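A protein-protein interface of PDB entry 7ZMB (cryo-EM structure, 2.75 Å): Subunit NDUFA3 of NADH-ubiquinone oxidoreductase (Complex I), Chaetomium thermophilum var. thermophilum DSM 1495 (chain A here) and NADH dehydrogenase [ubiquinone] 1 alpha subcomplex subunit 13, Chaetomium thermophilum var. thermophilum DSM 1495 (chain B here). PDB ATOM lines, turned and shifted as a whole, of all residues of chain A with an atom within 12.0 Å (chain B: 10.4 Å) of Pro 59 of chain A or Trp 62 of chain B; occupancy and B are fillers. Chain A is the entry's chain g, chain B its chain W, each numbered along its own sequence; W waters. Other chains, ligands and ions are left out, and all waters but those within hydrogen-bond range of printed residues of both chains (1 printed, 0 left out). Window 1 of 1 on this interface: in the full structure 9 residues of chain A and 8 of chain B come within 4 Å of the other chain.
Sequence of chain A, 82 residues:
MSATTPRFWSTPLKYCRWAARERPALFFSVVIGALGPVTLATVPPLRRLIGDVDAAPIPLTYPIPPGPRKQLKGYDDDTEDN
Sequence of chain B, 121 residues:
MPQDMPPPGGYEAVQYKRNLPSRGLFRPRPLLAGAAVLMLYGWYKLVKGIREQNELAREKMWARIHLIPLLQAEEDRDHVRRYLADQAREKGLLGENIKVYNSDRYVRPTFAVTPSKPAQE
Water W1 bridges ND1 of His 66 of chain B and OH of Tyr 62 of chain A.
The guanidinium group (NE) of Arg 58 of chain B lies within salt-bridge range of the side-chain carboxylate (OE2) of Glu 55 of chain B.
A ring nitrogen (NE2) of His 66 of chain B sits close to the backbone carbonyl oxygen of Trp 62 of chain B, at 3.4 Å.
SD of Met 61 of chain B sits close to O of Pro 59 of chain A.
The guanidinium group of Arg 58 of chain B lies within hydrogen-bond range of the backbone carbonyl oxygen of Ala 56 of chain A (3.0 Å).
Printed residues of chain A that touch a printed residue of chain B: Ala 55, Ala 56, Pro 57, Ile 58, Pro 59, Tyr 62 and Pro 63.
Hydrophobic or aromatic side chains of chain B within 4 Å of the printed part of chain A: Met 61, Trp 62, Ile 65, Ile 68 and Pro 69.
Pro 59 of chain A touches just these residues of chain B: Met 61, Trp 62 and Ile 65.
Trp 62 of chain B touches just these residues of chain A: Pro 59 (3.6 Å) and Pro 63 (3.6 Å).
Of chain A, only Ile 58 (3.9 Å) and Pro 59 (3.4 Å) come within 4 Å of Met 61 of chain B.
No residue of chain A comes within 4 Å of Ala 63 of chain B.
No residue of chain A comes within 4 Å of His 66 of chain B.
Of the printed residues of chain A, Asn 54 of chain B touches Ile 58.
Printed residues of chain A within 4 Å of Ile 68 of chain B: Tyr 62 (3.9 Å).
Printed residues of chain B within 4 Å of Pro 57 of chain A: Arg 58 (3.96 Å).
Printed residues of chain B within 4 Å of Ala 55 of chain A: Arg 58.
Printed residues of chain B within 4 Å of Ile 58 of chain A: Asn 54 (3.7 Å), Arg 58 (3.99 Å) and Met 61 (3.9 Å).
Ile 64 of chain A touches none of the printed residues of chain B.
The nearest residue of chain B that does not touch Pro 59 of chain A is Arg 58 of chain B (4.4 Å).
The nearest residue of chain A that does not touch Trp 62 of chain B is Ile 58 of chain A (6.3 Å).
Ala 55 of chain A touches Arg 58 of chain B.
Pro 57 of chain A touches Arg 58 of chain B (O to NH2, 3.96 Å).
O of Asn 54 of chain B touches CG2 of Ile 58 of chain A, at 3.7 Å.
Arg 58 of chain B touches Ile 58 of chain A.
CD1 of Ile 58 of chain A touches CG of Met 61 of chain B, at 3.9 Å.
Trp 62 of chain B touches Pro 59 of chain A.
Pro 59 of chain A touches Ile 65 of chain B.
CE2 of Tyr 62 of chain A touches O of Ile 65 of chain B (3.3 Å).
CG of Pro 63 of chain A touches CH2 of Trp 62 of chain B (3.6 Å).
CD of Pro 63 of chain A touches CD1 of Ile 65 of chain B (3.9 Å).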
ATOM      1  N   ALA A  55      23.792 -24.529  34.005  1.00  0.00           N
ATOM      2  CA  ALA A  55      23.640 -24.595  32.536  1.00  0.00           C
ATOM      3  C   ALA A  55      23.531 -23.191  31.946  1.00  0.00           C
ATOM      4  O   ALA A  55      23.218 -22.253  32.699  1.00  0.00           O
ATOM      5  CB  ALA A  55      22.462 -25.455  32.173  1.00  0.00           C
ATOM      6  N   ALA A  56      23.803 -23.058  30.649  1.00  0.00           N
ATOM      7  CA  ALA A  56      23.661 -21.750  29.966  1.00  0.00           C
ATOM      8  C   ALA A  56      22.176 -21.374  29.833  1.00  0.00           C
ATOM      9  O   ALA A  56      21.363 -22.302  29.683  1.00  0.00           O
ATOM     10  CB  ALA A  56      24.321 -21.809  28.620  1.00  0.00           C
ATOM     11  N   PRO A  57      21.752 -20.083  29.887  1.00  0.00           N
ATOM     12  CA  PRO A  57      20.343 -19.771  29.661  1.00  0.00           C
ATOM     13  C   PRO A  57      19.857 -20.181  28.258  1.00  0.00           C
ATOM     14  O   PRO A  57      20.553 -19.934  27.299  1.00  0.00           O
ATOM     15  CB  PRO A  57      20.311 -18.248  29.839  1.00  0.00           C
ATOM     16  CG  PRO A  57      21.725 -17.806  29.559  1.00  0.00           C
ATOM     17  CD  PRO A  57      22.572 -18.905  30.159  1.00  0.00           C
ATOM     18  N   ILE A  58      18.667 -20.784  28.176  1.00  0.00           N
ATOM     19  CA  ILE A  58      18.094 -21.229  26.867  1.00  0.00           C
ATOM     20  C   ILE A  58      17.642 -20.011  26.049  1.00  0.00           C
ATOM     21  O   ILE A  58      17.220 -19.017  26.656  1.00  0.00           O
ATOM     22  CB  ILE A  58      16.977 -22.268  27.075  1.00  0.00           C
ATOM     23  CG1 ILE A  58      15.694 -21.644  27.630  1.00  0.00           C
ATOM     24  CG2 ILE A  58      17.471 -23.418  27.936  1.00  0.00           C
ATOM     25  CD1 ILE A  58      14.434 -22.210  27.028  1.00  0.00           C
ATOM     26  N   PRO A  59      17.760 -20.013  24.707  1.00  0.00           N
ATOM     27  CA  PRO A  59      17.399 -18.830  23.916  1.00  0.00           C
ATOM     28  C   PRO A  59      15.887 -18.536  23.982  1.00  0.00           C
ATOM     29  O   PRO A  59      15.108 -19.440  23.810  1.00  0.00           O
ATOM     30  CB  PRO A  59      17.901 -19.196  22.512  1.00  0.00           C
ATOM     31  CG  PRO A  59      17.929 -20.706  22.486  1.00  0.00           C
ATOM     32  CD  PRO A  59      18.276 -21.116  23.900  1.00  0.00           C
ATOM     33  N   LEU A  60      15.508 -17.290  24.264  1.00  0.00           N
ATOM     34  CA  LEU A  60      14.075 -16.913  24.388  1.00  0.00           C
ATOM     35  C   LEU A  60      13.802 -15.806  23.379  1.00  0.00           C
ATOM     36  O   LEU A  60      12.625 -15.491  23.166  1.00  0.00           O
ATOM     37  CB  LEU A  60      13.764 -16.525  25.834  1.00  0.00           C
ATOM     38  CG  LEU A  60      13.849 -17.665  26.847  1.00  0.00           C
ATOM     39  CD1 LEU A  60      13.441 -17.201  28.232  1.00  0.00           C
ATOM     40  CD2 LEU A  60      12.980 -18.830  26.410  1.00  0.00           C
ATOM     41  N   THR A  61      14.834 -15.370  22.670  1.00  0.00           N
ATOM     42  CA  THR A  61      14.668 -14.414  21.547  1.00  0.00           C
ATOM     43  C   THR A  61      15.716 -14.834  20.518  1.00  0.00           C
ATOM     44  O   THR A  61      16.663 -15.535  20.907  1.00  0.00           O
ATOM     45  CB  THR A  61      14.914 -12.962  21.979  1.00  0.00           C
ATOM     46  OG1 THR A  61      14.513 -12.089  20.925  1.00  0.00           O
ATOM     47  CG2 THR A  61      16.357 -12.684  22.338  1.00  0.00           C
ATOM     48  N   TYR A  62      15.476 -14.545  19.242  1.00  0.00           N
ATOM     49  CA  TYR A  62      16.463 -14.901  18.196  1.00  0.00           C
ATOM     50  C   TYR A  62      17.801 -14.289  18.606  1.00  0.00           C
ATOM     51  O   TYR A  62      17.857 -13.103  18.954  1.00  0.00           O
ATOM     52  CB  TYR A  62      16.028 -14.397  16.819  1.00  0.00           C
ATOM     53  CG  TYR A  62      16.830 -14.948  15.666  1.00  0.00           C
ATOM     54  CD1 TYR A  62      18.067 -14.422  15.332  1.00  0.00           C
ATOM     55  CD2 TYR A  62      16.352 -16.002  14.907  1.00  0.00           C
ATOM     56  CE1 TYR A  62      18.816 -14.935  14.287  1.00  0.00           C
ATOM     57  CE2 TYR A  62      17.080 -16.518  13.851  1.00  0.00           C
ATOM     58  CZ  TYR A  62      18.318 -15.986  13.541  1.00  0.00           C
ATOM     59  OH  TYR A  62      19.031 -16.497  12.497  1.00  0.00           O
ATOM     60  N   PRO A  63      18.897 -15.068  18.568  1.00  0.00           N
ATOM     61  CA  PRO A  63      20.192 -14.559  18.974  1.00  0.00           C
ATOM     62  C   PRO A  63      20.763 -13.821  17.762  1.00  0.00           C
ATOM     63  O   PRO A  63      21.209 -14.456  16.843  1.00  0.00           O
ATOM     64  CB  PRO A  63      21.002 -15.833  19.254  1.00  0.00           C
ATOM     65  CG  PRO A  63      20.009 -16.974  19.154  1.00  0.00           C
ATOM     66  CD  PRO A  63      18.932 -16.483  18.216  1.00  0.00           C
ATOM     67  N   ILE A  64      20.727 -12.494  17.810  1.00  0.00           N
ATOM     68  CA  ILE A  64      21.231 -11.697  16.661  1.00  0.00           C
ATOM     69  C   ILE A  64      22.756 -11.756  16.724  1.00  0.00           C
ATOM     70  O   ILE A  64      23.291 -11.380  17.780  1.00  0.00           O
ATOM     71  CB  ILE A  64      20.689 -10.255  16.634  1.00  0.00           C
ATOM     72  CG1 ILE A  64      19.162 -10.221  16.541  1.00  0.00           C
ATOM     73  CG2 ILE A  64      21.342  -9.465  15.512  1.00  0.00           C
ATOM     74  CD1 ILE A  64      18.629 -10.565  15.177  1.00  0.00           C
ATOM     75  N   PRO A  65      23.490 -12.238  15.689  1.00  0.00           N
ATOM     76  CA  PRO A  65      24.934 -12.275  15.800  1.00  0.00           C
ATOM     77  C   PRO A  65      25.562 -10.875  15.904  1.00  0.00           C
ATOM     78  O   PRO A  65      25.009  -9.980  15.306  1.00  0.00           O
ATOM     79  CB  PRO A  65      25.331 -12.961  14.488  1.00  0.00           C
ATOM     80  CG  PRO A  65      24.102 -13.710  14.066  1.00  0.00           C
ATOM     81  CD  PRO A  65      22.987 -12.758  14.421  1.00  0.00           C
ATOM     82  N   PRO A  66      26.672 -10.627  16.650  1.00  0.00           N
ATOM     83  CA  PRO A  66      27.319  -9.316  16.599  1.00  0.00           C
ATOM     84  C   PRO A  66      28.331  -9.229  15.464  1.00  0.00           C
ATOM     85  O   PRO A  66      28.775 -10.235  14.905  1.00  0.00           O
ATOM     86  CB  PRO A  66      28.016  -9.228  17.962  1.00  0.00           C
ATOM     87  CG  PRO A  66      28.359 -10.653  18.283  1.00  0.00           C
ATOM     88  CD  PRO A  66      27.371 -11.549  17.561  1.00  0.00           C
ATOM     89  N   ASN B  54      15.002 -28.863  30.773  1.00  0.00           N
ATOM     90  CA  ASN B  54      15.599 -27.568  30.375  1.00  0.00           C
ATOM     91  C   ASN B  54      16.434 -27.803  29.120  1.00  0.00           C
ATOM     92  O   ASN B  54      16.420 -26.919  28.257  1.00  0.00           O
ATOM     93  CB  ASN B  54      16.323 -26.873  31.538  1.00  0.00           C
ATOM     94  CG  ASN B  54      15.395 -26.394  32.634  1.00  0.00           C
ATOM     95  OD1 ASN B  54      14.184 -26.590  32.568  1.00  0.00           O
ATOM     96  ND2 ASN B  54      15.956 -25.763  33.650  1.00  0.00           N
ATOM     97  N   GLU B  55      17.152 -28.929  29.044  1.00  0.00           N
ATOM     98  CA  GLU B  55      17.894 -29.305  27.816  1.00  0.00           C
ATOM     99  C   GLU B  55      16.929 -29.596  26.661  1.00  0.00           C
ATOM    100  O   GLU B  55      17.255 -29.227  25.526  1.00  0.00           O
ATOM    101  CB  GLU B  55      18.835 -30.461  28.141  1.00  0.00           C
ATOM    102  CG  GLU B  55      19.991 -30.020  29.007  1.00  0.00           C
ATOM    103  CD  GLU B  55      20.509 -28.653  28.602  1.00  0.00           C
ATOM    104  OE1 GLU B  55      20.508 -27.744  29.454  1.00  0.00           O
ATOM    105  OE2 GLU B  55      20.917 -28.504  27.434  1.00  0.00           O
ATOM    106  N   LEU B  56      15.800 -30.245  26.936  1.00  0.00           N
ATOM    107  CA  LEU B  56      14.769 -30.511  25.903  1.00  0.00           C
ATOM    108  C   LEU B  56      14.239 -29.167  25.415  1.00  0.00           C
ATOM    109  O   LEU B  56      13.995 -29.041  24.209  1.00  0.00           O
ATOM    110  CB  LEU B  56      13.653 -31.349  26.534  1.00  0.00           C
ATOM    111  CG  LEU B  56      13.942 -32.838  26.684  1.00  0.00           C
ATOM    112  CD1 LEU B  56      12.716 -33.556  27.220  1.00  0.00           C
ATOM    113  CD2 LEU B  56      14.368 -33.437  25.357  1.00  0.00           C
ATOM    114  N   ALA B  57      14.071 -28.212  26.332  1.00  0.00           N
ATOM    115  CA  ALA B  57      13.616 -26.849  25.981  1.00  0.00           C
ATOM    116  C   ALA B  57      14.639 -26.138  25.087  1.00  0.00           C
ATOM    117  O   ALA B  57      14.204 -25.431  24.176  1.00  0.00           O
ATOM    118  CB  ALA B  57      13.310 -26.083  27.237  1.00  0.00           C
ATOM    119  N   ARG B  58      15.941 -26.336  25.333  1.00  0.00           N
ATOM    120  CA  ARG B  58      17.009 -25.703  24.512  1.00  0.00           C
ATOM    121  C   ARG B  58      16.913 -26.180  23.059  1.00  0.00           C
ATOM    122  O   ARG B  58      17.054 -25.341  22.162  1.00  0.00           O
ATOM    123  CB  ARG B  58      18.386 -26.045  25.081  1.00  0.00           C
ATOM    124  CG  ARG B  58      19.547 -25.343  24.393  1.00  0.00           C
ATOM    125  CD  ARG B  58      20.884 -25.845  24.899  1.00  0.00           C
ATOM    126  NE  ARG B  58      20.927 -25.899  26.351  1.00  0.00           N
ATOM    127  CZ  ARG B  58      21.244 -24.880  27.138  1.00  0.00           C
ATOM    128  NH1 ARG B  58      21.248 -25.042  28.449  1.00  0.00           N
ATOM    129  NH2 ARG B  58      21.556 -23.707  26.620  1.00  0.00           N
ATOM    130  N   GLU B  59      16.678 -27.477  22.852  1.00  0.00           N
ATOM    131  CA  GLU B  59      16.565 -28.059  21.487  1.00  0.00           C
ATOM    132  C   GLU B  59      15.328 -27.514  20.768  1.00  0.00           C
ATOM    133  O   GLU B  59      15.450 -27.181  19.576  1.00  0.00           O
ATOM    134  CB  GLU B  59      16.599 -29.581  21.599  1.00  0.00           C
ATOM    135  CG  GLU B  59      16.353 -30.323  20.305  1.00  0.00           C
ATOM    136  CD  GLU B  59      16.084 -31.795  20.554  1.00  0.00           C
ATOM    137  OE1 GLU B  59      16.144 -32.580  19.595  1.00  0.00           O
ATOM    138  OE2 GLU B  59      15.811 -32.147  21.714  1.00  0.00           O
ATOM    139  N   LYS B  60      14.197 -27.401  21.469  1.00  0.00           N
ATOM    140  CA  LYS B  60      12.932 -26.916  20.842  1.00  0.00           C
ATOM    141  C   LYS B  60      13.116 -25.465  20.396  1.00  0.00           C
ATOM    142  O   LYS B  60      12.614 -25.118  19.325  1.00  0.00           O
ATOM    143  CB  LYS B  60      11.754 -27.051  21.810  1.00  0.00           C
ATOM    144  CG  LYS B  60      10.413 -26.546  21.307  1.00  0.00           C
ATOM    145  CD  LYS B  60       9.355 -26.598  22.375  1.00  0.00           C
ATOM    146  CE  LYS B  60       7.951 -26.615  21.821  1.00  0.00           C
ATOM    147  NZ  LYS B  60       6.993 -27.143  22.817  1.00  0.00           N
ATOM    148  N   MET B  61      13.845 -24.671  21.177  1.00  0.00           N
ATOM    149  CA  MET B  61      14.052 -23.239  20.845  1.00  0.00           C
ATOM    150  C   MET B  61      15.010 -23.083  19.658  1.00  0.00           C
ATOM    151  O   MET B  61      14.704 -22.261  18.783  1.00  0.00           O
ATOM    152  CB  MET B  61      14.556 -22.463  22.063  1.00  0.00           C
ATOM    153  CG  MET B  61      13.553 -22.366  23.193  1.00  0.00           C
ATOM    154  SD  MET B  61      12.174 -21.245  22.848  1.00  0.00           S
ATOM    155  CE  MET B  61      10.910 -22.404  22.326  1.00  0.00           C
ATOM    156  N   TRP B  62      16.105 -23.848  19.616  1.00  0.00           N
ATOM    157  CA  TRP B  62      17.038 -23.791  18.459  1.00  0.00           C
ATOM    158  C   TRP B  62      16.364 -24.289  17.175  1.00  0.00           C
ATOM    159  O   TRP B  62      16.659 -23.728  16.117  1.00  0.00           O
ATOM    160  CB  TRP B  62      18.381 -24.462  18.764  1.00  0.00           C
ATOM    161  CG  TRP B  62      19.318 -23.594  19.543  1.00  0.00           C
ATOM    162  CD1 TRP B  62      19.673 -23.735  20.852  1.00  0.00           C
ATOM    163  CD2 TRP B  62      20.011 -22.430  19.064  1.00  0.00           C
ATOM    164  NE1 TRP B  62      20.544 -22.747  21.218  1.00  0.00           N
ATOM    165  CE2 TRP B  62      20.768 -21.928  20.144  1.00  0.00           C
ATOM    166  CE3 TRP B  62      20.071 -21.766  17.834  1.00  0.00           C
ATOM    167  CZ2 TRP B  62      21.571 -20.797  20.026  1.00  0.00           C
ATOM    168  CZ3 TRP B  62      20.865 -20.648  17.720  1.00  0.00           C
ATOM    169  CH2 TRP B  62      21.608 -20.175  18.801  1.00  0.00           C
ATOM    170  N   ALA B  63      15.456 -25.255  17.275  1.00  0.00           N
ATOM    171  CA  ALA B  63      14.726 -25.788  16.103  1.00  0.00           C
ATOM    172  C   ALA B  63      13.795 -24.695  15.582  1.00  0.00           C
ATOM    173  O   ALA B  63      13.669 -24.558  14.354  1.00  0.00           O
ATOM    174  CB  ALA B  63      13.943 -27.016  16.475  1.00  0.00           C
ATOM    175  N   ARG B  64      13.202 -23.923  16.489  1.00  0.00           N
ATOM    176  CA  ARG B  64      12.318 -22.802  16.081  1.00  0.00           C
ATOM    177  C   ARG B  64      13.144 -21.651  15.495  1.00  0.00           C
ATOM    178  O   ARG B  64      12.691 -21.068  14.511  1.00  0.00           O
ATOM    179  CB  ARG B  64      11.433 -22.359  17.249  1.00  0.00           C
ATOM    180  CG  ARG B  64      10.338 -23.344  17.624  1.00  0.00           C
ATOM    181  CD  ARG B  64       9.412 -22.739  18.652  1.00  0.00           C
ATOM    182  NE  ARG B  64       8.277 -23.607  18.905  1.00  0.00           N
ATOM    183  CZ  ARG B  64       7.270 -23.305  19.709  1.00  0.00           C
ATOM    184  NH1 ARG B  64       6.276 -24.160  19.874  1.00  0.00           N
ATOM    185  NH2 ARG B  64       7.254 -22.143  20.337  1.00  0.00           N
ATOM    186  N   ILE B  65      14.317 -21.369  16.056  1.00  0.00           N
ATOM    187  CA  ILE B  65      15.170 -20.235  15.598  1.00  0.00           C
ATOM    188  C   ILE B  65      15.573 -20.442  14.133  1.00  0.00           C
ATOM    189  O   ILE B  65      15.574 -19.450  13.397  1.00  0.00           O
ATOM    190  CB  ILE B  65      16.372 -20.049  16.548  1.00  0.00           C
ATOM    191  CG1 ILE B  65      16.016 -19.158  17.739  1.00  0.00           C
ATOM    192  CG2 ILE B  65      17.599 -19.539  15.811  1.00  0.00           C
ATOM    193  CD1 ILE B  65      16.711 -19.550  19.015  1.00  0.00           C
ATOM    194  N   HIS B  66      15.836 -21.681  13.711  1.00  0.00           N
ATOM    195  CA  HIS B  66      16.173 -21.968  12.289  1.00  0.00           C
ATOM    196  C   HIS B  66      14.978 -21.667  11.367  1.00  0.00           C
ATOM    197  O   HIS B  66      15.204 -21.170  10.256  1.00  0.00           O
ATOM    198  CB  HIS B  66      16.720 -23.393  12.137  1.00  0.00           C
ATOM    199  CG  HIS B  66      17.895 -23.713  12.999  1.00  0.00           C
ATOM    200  ND1 HIS B  66      18.900 -22.802  13.255  1.00  0.00           N
ATOM    201  CD2 HIS B  66      18.242 -24.848  13.643  1.00  0.00           C
ATOM    202  CE1 HIS B  66      19.804 -23.358  14.034  1.00  0.00           C
ATOM    203  NE2 HIS B  66      19.425 -24.611  14.286  1.00  0.00           N
ATOM    204  N   LEU B  67      13.770 -22.029  11.773  1.00  0.00           N
ATOM    205  CA  LEU B  67      12.552 -21.801  10.957  1.00  0.00           C
ATOM    206  C   LEU B  67      12.146 -20.326  10.922  1.00  0.00           C
ATOM    207  O   LEU B  67      11.533 -19.925   9.931  1.00  0.00           O
ATOM    208  CB  LEU B  67      11.451 -22.718  11.489  1.00  0.00           C
ATOM    209  CG  LEU B  67      11.823 -24.193  11.417  1.00  0.00           C
ATOM    210  CD1 LEU B  67      10.923 -25.037  12.300  1.00  0.00           C
ATOM    211  CD2 LEU B  67      11.821 -24.672   9.977  1.00  0.00           C
ATOM    212  N   ILE B  68      12.488 -19.555  11.952  1.00  0.00           N
ATOM    213  CA  ILE B  68      12.041 -18.138  12.065  1.00  0.00           C
ATOM    214  C   ILE B  68      12.369 -17.319  10.814  1.00  0.00           C
ATOM    215  O   ILE B  68      11.461 -16.597  10.380  1.00  0.00           O
ATOM    216  CB  ILE B  68      12.595 -17.492  13.357  1.00  0.00           C
ATOM    217  CG1 ILE B  68      11.742 -17.804  14.587  1.00  0.00           C
ATOM    218  CG2 ILE B  68      12.809 -15.996  13.194  1.00  0.00           C
ATOM    219  CD1 ILE B  68      12.279 -17.213  15.867  1.00  0.00           C
ATOM    220  N   PRO B  69      13.570 -17.343  10.182  1.00  0.00           N
ATOM    221  CA  PRO B  69      13.845 -16.400   9.087  1.00  0.00           C
ATOM    222  C   PRO B  69      13.129 -16.689   7.770  1.00  0.00           C
ATOM    223  O   PRO B  69      12.761 -15.757   7.141  1.00  0.00           O
ATOM    224  CB  PRO B  69      15.369 -16.438   8.901  1.00  0.00           C
ATOM    225  CG  PRO B  69      15.856 -17.047  10.196  1.00  0.00           C
ATOM    226  CD  PRO B  69      14.789 -18.060  10.546  1.00  0.00           C
ATOM    227  N   LEU B  70      12.917 -17.959   7.430  1.00  0.00           N
ATOM    228  CA  LEU B  70      12.166 -18.317   6.197  1.00  0.00           C
ATOM    229  C   LEU B  70      10.668 -18.094   6.399  1.00  0.00           C
ATOM    230  O   LEU B  70       9.988 -17.783   5.409  1.00  0.00           O
ATOM    231  CB  LEU B  70      12.504 -19.753   5.788  1.00  0.00           C
ATOM    232  CG  LEU B  70      12.260 -20.839   6.836  1.00  0.00           C
ATOM    233  CD1 LEU B  70      10.989 -21.619   6.534  1.00  0.00           C
ATOM    234  CD2 LEU B  70      13.446 -21.787   6.914  1.00  0.00           C
HETATM  235  O   HOH W   1      18.990 -19.739  12.303  1.00  0.00           O
